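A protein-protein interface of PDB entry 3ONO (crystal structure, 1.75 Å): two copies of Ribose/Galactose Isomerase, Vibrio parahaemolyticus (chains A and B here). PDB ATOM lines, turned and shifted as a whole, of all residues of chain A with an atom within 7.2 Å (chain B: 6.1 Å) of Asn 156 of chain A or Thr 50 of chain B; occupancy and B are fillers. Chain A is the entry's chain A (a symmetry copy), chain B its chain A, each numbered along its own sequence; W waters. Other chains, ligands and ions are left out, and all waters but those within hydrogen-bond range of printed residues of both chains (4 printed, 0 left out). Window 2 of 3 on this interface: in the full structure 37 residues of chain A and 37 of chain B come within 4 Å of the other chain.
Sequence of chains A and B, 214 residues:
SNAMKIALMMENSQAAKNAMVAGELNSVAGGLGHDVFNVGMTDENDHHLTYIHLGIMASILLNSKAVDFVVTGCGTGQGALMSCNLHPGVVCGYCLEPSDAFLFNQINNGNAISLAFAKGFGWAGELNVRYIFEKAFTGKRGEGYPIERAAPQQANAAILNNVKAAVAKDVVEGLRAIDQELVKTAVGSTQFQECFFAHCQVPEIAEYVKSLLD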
ATOM      1  N   ILE A 107      -7.562   4.313 -25.946  1.00  0.00           N
ATOM      2  CA  ILE A 107      -8.334   4.908 -24.856  1.00  0.00           C
ATOM      3  C   ILE A 107      -8.998   3.832 -24.002  1.00  0.00           C
ATOM      4  O   ILE A 107      -8.908   3.847 -22.762  1.00  0.00           O
ATOM      5  CB  ILE A 107      -9.427   5.860 -25.396  1.00  0.00           C
ATOM      6  CG1 ILE A 107      -8.802   7.054 -26.161  1.00  0.00           C
ATOM      7  CG2 ILE A 107     -10.364   6.325 -24.258  1.00  0.00           C
ATOM      8  CD1 ILE A 107      -9.886   7.887 -26.850  1.00  0.00           C
ATOM      9  N   ASN A 108      -9.656   2.884 -24.660  1.00  0.00           N
ATOM     10  CA  ASN A 108     -10.419   1.885 -23.935  1.00  0.00           C
ATOM     11  C   ASN A 108      -9.653   0.584 -23.708  1.00  0.00           C
ATOM     12  O   ASN A 108      -9.854  -0.091 -22.692  1.00  0.00           O
ATOM     13  CB  ASN A 108     -11.719   1.615 -24.692  1.00  0.00           C
ATOM     14  CG  ASN A 108     -12.433   2.897 -25.055  1.00  0.00           C
ATOM     15  OD1 ASN A 108     -12.351   3.364 -26.193  1.00  0.00           O
ATOM     16  ND2 ASN A 108     -13.112   3.495 -24.078  1.00  0.00           N
ATOM     17  N   ALA A 150      -2.714   9.680 -20.890  1.00  0.00           N
ATOM     18  CA  ALA A 150      -3.081   8.289 -20.737  1.00  0.00           C
ATOM     19  C   ALA A 150      -3.544   7.937 -19.320  1.00  0.00           C
ATOM     20  O   ALA A 150      -4.212   6.925 -19.146  1.00  0.00           O
ATOM     21  CB  ALA A 150      -1.924   7.385 -21.161  1.00  0.00           C
ATOM     22  N   ALA A 151      -3.208   8.752 -18.316  1.00  0.00           N
ATOM     23  CA  ALA A 151      -3.436   8.296 -16.914  1.00  0.00           C
ATOM     24  C   ALA A 151      -4.904   8.064 -16.539  1.00  0.00           C
ATOM     25  O   ALA A 151      -5.272   6.963 -16.111  1.00  0.00           O
ATOM     26  CB  ALA A 151      -2.770   9.231 -15.902  1.00  0.00           C
ATOM     27  N   PRO A 152      -5.749   9.099 -16.659  1.00  0.00           N
ATOM     28  CA  PRO A 152      -7.151   8.867 -16.286  1.00  0.00           C
ATOM     29  C   PRO A 152      -7.851   7.871 -17.205  1.00  0.00           C
ATOM     30  O   PRO A 152      -8.750   7.154 -16.751  1.00  0.00           O
ATOM     31  CB  PRO A 152      -7.792  10.255 -16.416  1.00  0.00           C
ATOM     32  CG  PRO A 152      -6.637  11.228 -16.450  1.00  0.00           C
ATOM     33  CD  PRO A 152      -5.492  10.492 -17.068  1.00  0.00           C
ATOM     34  N   GLN A 153      -7.480   7.829 -18.480  1.00  0.00           N
ATOM     35  CA  GLN A 153      -8.090   6.862 -19.400  1.00  0.00           C
ATOM     36  C   GLN A 153      -7.752   5.440 -18.970  1.00  0.00           C
ATOM     37  O   GLN A 153      -8.609   4.562 -18.953  1.00  0.00           O
ATOM     38  CB  GLN A 153      -7.615   7.101 -20.827  1.00  0.00           C
ATOM     39  CG  GLN A 153      -8.223   8.366 -21.402  1.00  0.00           C
ATOM     40  CD  GLN A 153      -7.655   8.741 -22.742  1.00  0.00           C
ATOM     41  OE1 GLN A 153      -6.664   8.163 -23.204  1.00  0.00           O
ATOM     42  NE2 GLN A 153      -8.272   9.733 -23.376  1.00  0.00           N
ATOM     43  N   GLN A 154      -6.483   5.219 -18.648  1.00  0.00           N
ATOM     44  CA  GLN A 154      -6.054   3.908 -18.160  1.00  0.00           C
ATOM     45  C   GLN A 154      -6.733   3.550 -16.837  1.00  0.00           C
ATOM     46  O   GLN A 154      -7.110   2.387 -16.603  1.00  0.00           O
ATOM     47  CB  GLN A 154      -4.529   3.871 -18.014  1.00  0.00           C
ATOM     48  CG  GLN A 154      -3.809   3.829 -19.369  1.00  0.00           C
ATOM     49  CD  GLN A 154      -2.324   4.167 -19.279  1.00  0.00           C
ATOM     50  OE1 GLN A 154      -1.828   4.604 -18.239  1.00  0.00           O
ATOM     51  NE2 GLN A 154      -1.610   3.980 -20.386  1.00  0.00           N
ATOM     52  N   ALA A 155      -6.856   4.536 -15.951  1.00  0.00           N
ATOM     53  CA  ALA A 155      -7.492   4.293 -14.656  1.00  0.00           C
ATOM     54  C   ALA A 155      -8.946   3.894 -14.833  1.00  0.00           C
ATOM     55  O   ALA A 155      -9.432   2.962 -14.178  1.00  0.00           O
ATOM     56  CB  ALA A 155      -7.384   5.531 -13.771  1.00  0.00           C
ATOM     57  N   ASN A 156      -9.646   4.583 -15.724  1.00  0.00           N
ATOM     58  CA  ASN A 156     -11.068   4.300 -15.885  1.00  0.00           C
ATOM     59  C   ASN A 156     -11.296   2.985 -16.592  1.00  0.00           C
ATOM     60  O   ASN A 156     -12.261   2.259 -16.288  1.00  0.00           O
ATOM     61  CB  ASN A 156     -11.770   5.466 -16.602  1.00  0.00           C
ATOM     62  CG  ASN A 156     -11.880   6.688 -15.696  1.00  0.00           C
ATOM     63  OD1 ASN A 156     -11.954   6.540 -14.461  1.00  0.00           O
ATOM     64  ND2 ASN A 156     -11.903   7.886 -16.286  1.00  0.00           N
ATOM     65  N   ALA A 157     -10.419   2.668 -17.538  1.00  0.00           N
ATOM     66  CA  ALA A 157     -10.532   1.395 -18.238  1.00  0.00           C
ATOM     67  C   ALA A 157     -10.338   0.248 -17.238  1.00  0.00           C
ATOM     68  O   ALA A 157     -11.033  -0.772 -17.310  1.00  0.00           O
ATOM     69  CB  ALA A 157      -9.518   1.309 -19.386  1.00  0.00           C
ATOM     70  N   ALA A 158      -9.414   0.415 -16.293  1.00  0.00           N
ATOM     71  CA  ALA A 158      -9.215  -0.624 -15.269  1.00  0.00           C
ATOM     72  C   ALA A 158     -10.456  -0.792 -14.399  1.00  0.00           C
ATOM     73  O   ALA A 158     -10.886  -1.910 -14.086  1.00  0.00           O
ATOM     74  CB  ALA A 158      -8.007  -0.273 -14.410  1.00  0.00           C
ATOM     75  N   ILE A 159     -11.020   0.331 -13.979  1.00  0.00           N
ATOM     76  CA  ILE A 159     -12.215   0.307 -13.156  1.00  0.00           C
ATOM     77  C   ILE A 159     -13.389  -0.356 -13.892  1.00  0.00           C
ATOM     78  O   ILE A 159     -14.146  -1.129 -13.285  1.00  0.00           O
ATOM     79  CB  ILE A 159     -12.555   1.730 -12.659  1.00  0.00           C
ATOM     80  CG1 ILE A 159     -11.481   2.181 -11.665  1.00  0.00           C
ATOM     81  CG2 ILE A 159     -13.939   1.778 -12.015  1.00  0.00           C
ATOM     82  CD1 ILE A 159     -11.506   3.684 -11.342  1.00  0.00           C
ATOM     83  N   LEU A 160     -13.515  -0.106 -15.195  1.00  0.00           N
ATOM     84  CA  LEU A 160     -14.603  -0.710 -15.959  1.00  0.00           C
ATOM     85  C   LEU A 160     -14.586  -2.226 -15.753  1.00  0.00           C
ATOM     86  O   LEU A 160     -15.625  -2.840 -15.564  1.00  0.00           O
ATOM     87  CB  LEU A 160     -14.510  -0.369 -17.465  1.00  0.00           C
ATOM     88  CG  LEU A 160     -15.592  -1.007 -18.345  1.00  0.00           C
ATOM     89  CD1 LEU A 160     -16.971  -0.456 -17.969  1.00  0.00           C
ATOM     90  CD2 LEU A 160     -15.301  -0.742 -19.810  1.00  0.00           C
ATOM     91  N   ASN A 161     -13.405  -2.832 -15.797  1.00  0.00           N
ATOM     92  CA  ASN A 161     -13.327  -4.279 -15.632  1.00  0.00           C
ATOM     93  C   ASN A 161     -13.821  -4.702 -14.257  1.00  0.00           C
ATOM     94  O   ASN A 161     -14.489  -5.740 -14.110  1.00  0.00           O
ATOM     95  CB  ASN A 161     -11.893  -4.778 -15.816  1.00  0.00           C
ATOM     96  CG  ASN A 161     -11.405  -4.622 -17.250  1.00  0.00           C
ATOM     97  OD1 ASN A 161     -12.195  -4.562 -18.179  1.00  0.00           O
ATOM     98  ND2 ASN A 161     -10.090  -4.567 -17.423  1.00  0.00           N
ATOM     99  N   ASN A 162     -13.455  -3.930 -13.235  1.00  0.00           N
ATOM    100  CA  ASN A 162     -13.903  -4.234 -11.865  1.00  0.00           C
ATOM    101  C   ASN A 162     -15.420  -4.191 -11.747  1.00  0.00           C
ATOM    102  O   ASN A 162     -16.045  -5.042 -11.094  1.00  0.00           O
ATOM    103  CB  ASN A 162     -13.395  -3.207 -10.862  1.00  0.00           C
ATOM    104  CG  ASN A 162     -11.896  -3.066 -10.851  1.00  0.00           C
ATOM    105  OD1 ASN A 162     -11.155  -3.940 -11.291  1.00  0.00           O
ATOM    106  ND2 ASN A 162     -11.443  -1.971 -10.293  1.00  0.00           N
ATOM    107  N   GLU B  11     -20.173  13.366 -18.374  1.00  0.00           N
ATOM    108  CA  GLU B  11     -19.035  13.222 -17.467  1.00  0.00           C
ATOM    109  C   GLU B  11     -17.974  14.314 -17.689  1.00  0.00           C
ATOM    110  O   GLU B  11     -18.176  15.234 -18.480  1.00  0.00           O
ATOM    111  CB  GLU B  11     -18.406  11.824 -17.573  1.00  0.00           C
ATOM    112  CG  GLU B  11     -18.103  11.388 -19.013  1.00  0.00           C
ATOM    113  CD  GLU B  11     -17.032  12.227 -19.685  1.00  0.00           C
ATOM    114  OE1 GLU B  11     -17.396  13.007 -20.573  1.00  0.00           O
ATOM    115  OE2 GLU B  11     -15.841  12.103 -19.335  1.00  0.00           O
ATOM    116  N   ASN B  12     -16.864  14.217 -16.949  1.00  0.00           N
ATOM    117  CA  ASN B  12     -15.956  15.357 -16.822  1.00  0.00           C
ATOM    118  C   ASN B  12     -15.293  15.784 -18.128  1.00  0.00           C
ATOM    119  O   ASN B  12     -15.110  16.984 -18.384  1.00  0.00           O
ATOM    120  CB  ASN B  12     -14.915  15.111 -15.719  1.00  0.00           C
ATOM    121  CG  ASN B  12     -13.875  14.088 -16.119  1.00  0.00           C
ATOM    122  OD1 ASN B  12     -12.866  14.432 -16.755  1.00  0.00           O
ATOM    123  ND2 ASN B  12     -14.112  12.816 -15.767  1.00  0.00           N
ATOM    124  N   MET B  41     -23.070  15.892 -14.984  1.00  0.00           N
ATOM    125  CA  MET B  41     -22.377  17.167 -14.818  1.00  0.00           C
ATOM    126  C   MET B  41     -22.988  18.287 -15.649  1.00  0.00           C
ATOM    127  O   MET B  41     -23.390  18.085 -16.795  1.00  0.00           O
ATOM    128  CB  MET B  41     -20.896  17.023 -15.138  1.00  0.00           C
ATOM    129  CG  MET B  41     -20.183  16.153 -14.120  1.00  0.00           C
ATOM    130  SD  MET B  41     -18.295  16.017 -14.485  1.00  0.00           S
ATOM    131  CE  MET B  41     -17.726  17.748 -13.792  1.00  0.00           C
ATOM    132  N   HIS B  48     -18.024  15.936  -9.572  1.00  0.00           N
ATOM    133  CA  HIS B  48     -17.192  15.269 -10.586  1.00  0.00           C
ATOM    134  C   HIS B  48     -17.637  13.826 -10.854  1.00  0.00           C
ATOM    135  O   HIS B  48     -17.865  13.055  -9.913  1.00  0.00           O
ATOM    136  CB  HIS B  48     -15.727  15.289 -10.136  1.00  0.00           C
ATOM    137  CG  HIS B  48     -14.758  14.860 -11.191  1.00  0.00           C
ATOM    138  ND1 HIS B  48     -14.391  13.544 -11.379  1.00  0.00           N
ATOM    139  CD2 HIS B  48     -14.058  15.580 -12.098  1.00  0.00           C
ATOM    140  CE1 HIS B  48     -13.522  13.473 -12.373  1.00  0.00           C
ATOM    141  NE2 HIS B  48     -13.300  14.694 -12.823  1.00  0.00           N
ATOM    142  N   LEU B  49     -17.744  13.483 -12.142  1.00  0.00           N
ATOM    143  CA  LEU B  49     -18.164  12.162 -12.601  1.00  0.00           C
ATOM    144  C   LEU B  49     -17.265  11.669 -13.736  1.00  0.00           C
ATOM    145  O   LEU B  49     -16.762  12.470 -14.542  1.00  0.00           O
ATOM    146  CB  LEU B  49     -19.581  12.249 -13.164  1.00  0.00           C
ATOM    147  CG  LEU B  49     -20.715  12.688 -12.244  1.00  0.00           C
ATOM    148  CD1 LEU B  49     -22.012  12.639 -13.041  1.00  0.00           C
ATOM    149  CD2 LEU B  49     -20.791  11.759 -11.027  1.00  0.00           C
ATOM    150  N   THR B  50     -17.099  10.353 -13.835  1.00  0.00           N
ATOM    151  CA  THR B  50     -16.474   9.769 -15.024  1.00  0.00           C
ATOM    152  C   THR B  50     -17.511   8.909 -15.727  1.00  0.00           C
ATOM    153  O   THR B  50     -18.626   8.721 -15.225  1.00  0.00           O
ATOM    154  CB  THR B  50     -15.332   8.808 -14.675  1.00  0.00           C
ATOM    155  OG1 THR B  50     -15.884   7.608 -14.122  1.00  0.00           O
ATOM    156  CG2 THR B  50     -14.365   9.422 -13.685  1.00  0.00           C
ATOM    157  N   TYR B  51     -17.131   8.323 -16.855  1.00  0.00           N
ATOM    158  CA  TYR B  51     -18.084   7.458 -17.545  1.00  0.00           C
ATOM    159  C   TYR B  51     -18.431   6.202 -16.753  1.00  0.00           C
ATOM    160  O   TYR B  51     -19.438   5.563 -17.044  1.00  0.00           O
ATOM    161  CB  TYR B  51     -17.616   7.102 -18.965  1.00  0.00           C
ATOM    162  CG  TYR B  51     -16.359   6.272 -19.053  1.00  0.00           C
ATOM    163  CD1 TYR B  51     -16.389   4.890 -18.829  1.00  0.00           C
ATOM    164  CD2 TYR B  51     -15.134   6.863 -19.409  1.00  0.00           C
ATOM    165  CE1 TYR B  51     -15.240   4.122 -18.955  1.00  0.00           C
ATOM    166  CE2 TYR B  51     -13.976   6.099 -19.522  1.00  0.00           C
ATOM    167  CZ  TYR B  51     -14.037   4.730 -19.275  1.00  0.00           C
ATOM    168  OH  TYR B  51     -12.906   3.949 -19.397  1.00  0.00           O
ATOM    169  N   ILE B  52     -17.637   5.857 -15.732  1.00  0.00           N
ATOM    170  CA  ILE B  52     -18.002   4.749 -14.866  1.00  0.00           C
ATOM    171  C   ILE B  52     -19.251   5.101 -14.065  1.00  0.00           C
ATOM    172  O   ILE B  52     -20.191   4.312 -13.965  1.00  0.00           O
ATOM    173  CB  ILE B  52     -16.862   4.391 -13.859  1.00  0.00           C
ATOM    174  CG1 ILE B  52     -15.597   3.981 -14.609  1.00  0.00           C
ATOM    175  CG2 ILE B  52     -17.319   3.250 -12.910  1.00  0.00           C
ATOM    176  CD1 ILE B  52     -15.751   2.739 -15.483  1.00  0.00           C
ATOM    177  N   HIS B  53     -19.273   6.299 -13.490  1.00  0.00           N
ATOM    178  CA  HIS B  53     -20.417   6.715 -12.694  1.00  0.00           C
ATOM    179  C   HIS B  53     -21.658   6.806 -13.570  1.00  0.00           C
ATOM    180  O   HIS B  53     -22.757   6.508 -13.117  1.00  0.00           O
ATOM    181  CB  HIS B  53     -20.150   8.055 -12.016  1.00  0.00           C
ATOM    182  CG  HIS B  53     -18.914   8.051 -11.172  1.00  0.00           C
ATOM    183  ND1 HIS B  53     -17.775   8.753 -11.519  1.00  0.00           N
ATOM    184  CD2 HIS B  53     -18.629   7.408 -10.012  1.00  0.00           C
ATOM    185  CE1 HIS B  53     -16.847   8.554 -10.596  1.00  0.00           C
ATOM    186  NE2 HIS B  53     -17.340   7.738  -9.670  1.00  0.00           N
ATOM    187  N   LEU B  54     -21.482   7.222 -14.823  1.00  0.00           N
ATOM    188  CA  LEU B  54     -22.634   7.328 -15.711  1.00  0.00           C
ATOM    189  C   LEU B  54     -23.409   6.011 -15.814  1.00  0.00           C
ATOM    190  O   LEU B  54     -24.652   5.999 -15.781  1.00  0.00           O
ATOM    191  CB  LEU B  54     -22.203   7.800 -17.116  1.00  0.00           C
ATOM    192  CG  LEU B  54     -21.536   9.176 -17.187  1.00  0.00           C
ATOM    193  CD1 LEU B  54     -21.155   9.516 -18.647  1.00  0.00           C
ATOM    194  CD2 LEU B  54     -22.431  10.278 -16.605  1.00  0.00           C
ATOM    195  N   GLY B  55     -22.702   4.907 -15.994  1.00  0.00           N
ATOM    196  CA  GLY B  55     -23.372   3.625 -16.120  1.00  0.00           C
ATOM    197  C   GLY B  55     -24.161   3.280 -14.865  1.00  0.00           C
ATOM    198  O   GLY B  55     -25.283   2.753 -14.931  1.00  0.00           O
ATOM    199  N   MET B  57     -25.373   5.386 -12.623  1.00  0.00           N
ATOM    200  CA  MET B  57     -26.527   6.289 -12.642  1.00  0.00           C
ATOM    201  C   MET B  57     -27.606   5.821 -13.606  1.00  0.00           C
ATOM    202  O   MET B  57     -28.796   5.863 -13.284  1.00  0.00           O
ATOM    203  CB  MET B  57     -26.081   7.723 -12.982  1.00  0.00           C
ATOM    204  CG  MET B  57     -25.057   8.218 -11.989  1.00  0.00           C
ATOM    205  SD  MET B  57     -24.006   9.708 -12.638  1.00  0.00           S
ATOM    206  CE  MET B  57     -25.322  11.041 -12.195  1.00  0.00           C
ATOM    207  N   LEU B 182     -17.659   4.328  -5.645  1.00  0.00           N
ATOM    208  CA  LEU B 182     -18.184   4.654  -6.970  1.00  0.00           C
ATOM    209  C   LEU B 182     -19.666   4.945  -6.888  1.00  0.00           C
ATOM    210  O   LEU B 182     -20.135   5.903  -7.478  1.00  0.00           O
ATOM    211  CB  LEU B 182     -17.964   3.521  -7.962  1.00  0.00           C
ATOM    212  CG  LEU B 182     -16.545   3.241  -8.439  1.00  0.00           C
ATOM    213  CD1 LEU B 182     -16.551   1.971  -9.264  1.00  0.00           C
ATOM    214  CD2 LEU B 182     -15.990   4.414  -9.272  1.00  0.00           C
HETATM  215  O   HOH W   1     -14.098   6.188 -12.635  1.00  0.00           O
HETATM  216  O   HOH W   2     -10.755   5.036 -20.544  1.00  0.00           O
HETATM  217  O   HOH W   3     -11.713  10.853 -15.729  1.00  0.00           O
HETATM  218  O   HOH W   4     -13.427   2.178 -21.564  1.00  0.00           O
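The backbone NH (N) of Ala 157 of chain A sits at hydrogen-bond distance from the side-chain hydroxyl (OH) of Tyr 51 of chain B (3.4 Å).
N of Thr 50 of chain B sits at hydrogen-bond distance from ND1 of His 53 of chain B (2.9 Å). ND2 of Asn 156 of chain A lies within hydrogen-bond range of O of Pro 152 of chain A, 3.3 Å away. The side-chain hydroxyl (OG1) of Thr 50 of chain B sits at hydrogen-bond distance from the backbone NH (N) of Ile 52 of chain B (3.0 Å).
Asn 156 of chain A touches Thr 50 of chain B. Asn 156 of chain A touches Tyr 51 of chain B. Asn 156 of chain A touches Ile 52 of chain B (O to CD1, 3.6 Å). CG1 of Ile 52 of chain B touches CG2 of Ile 159 of chain A, 3.8 Å away. Ile 159 of chain A touches Leu 182 of chain B (CG2 to CD1, 3.8 Å). Leu 160 of chain A touches Ile 52 of chain B (N to CD1, 3.6 Å).
Of chain B, only Thr 50, Tyr 51 and Ile 52 come within 4 Å of Asn 156 of chain A. Of the printed residues of chain B, Ala 157 of chain A touches Tyr 51 (3.4 Å). Printed residues of chain B within 4 Å of Ile 159 of chain A: Ile 52 (3.8 Å) and Leu 182 (3.8 Å). Thr 50 of chain B touches just one residue of chain A: Asn 156. Of the printed residues of chain A, Ile 52 of chain B touches Asn 156, Ile 159 and Leu 160. The nearest residue of chain B that does not touch Asn 156 of chain A is Asn 12 of chain B (5.4 Å). The nearest residue of chain A that does not touch Thr 50 of chain B is Ile 159 of chain A (6.5 Å).
Printed residues of chain A that touch a printed residue of chain B: Asn 156, Ala 157, Ile 159 and Leu 160. Along chain A the printed residues that touch a printed residue of chain B span positions 156 to 160. Of the 13 printed residues of chain B, 4 touch a printed residue of chain A. Hydrophobic or aromatic side chains of chain B that line the printed part of chain A: Tyr 51, Ile 52 and Leu 182. Among the printed residues, 7 pairs touch across the chains. Among the printed residues, no Asp or Glu carboxylate lies within 4 Å of a Lys or Arg side-chain nitrogen of the other chain.
No position is printed for both chains.
Water W2 lies within hydrogen-bond range of the side-chain hydroxyl (OH) of Tyr 51 of chain B (2.7 Å), the backbone carbonyl oxygen (O) of Gln 153 of chain A (2.7 Å) and the backbone carbonyl oxygen (O) of Ile 107 of chain A (3.1 Å). Water W1 bridges OG1 of Thr 50 of chain B (2.7 Å) and OD1 of Asn 156 of chain A (2.8 Å). Water W4 lies within hydrogen-bond range of the side-chain hydroxyl of Tyr 51 of chain B (2.8 Å) and the side-chain amide nitrogen of Asn 108 of chain A (2.9 Å). Water W3 lies within hydrogen-bond range of the side-chain amide nitrogen (ND2) of Asn 156 of chain A (3.0 Å) and the side-chain amide nitrogen (ND2) of Asn 12 of chain B (3.1 Å).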
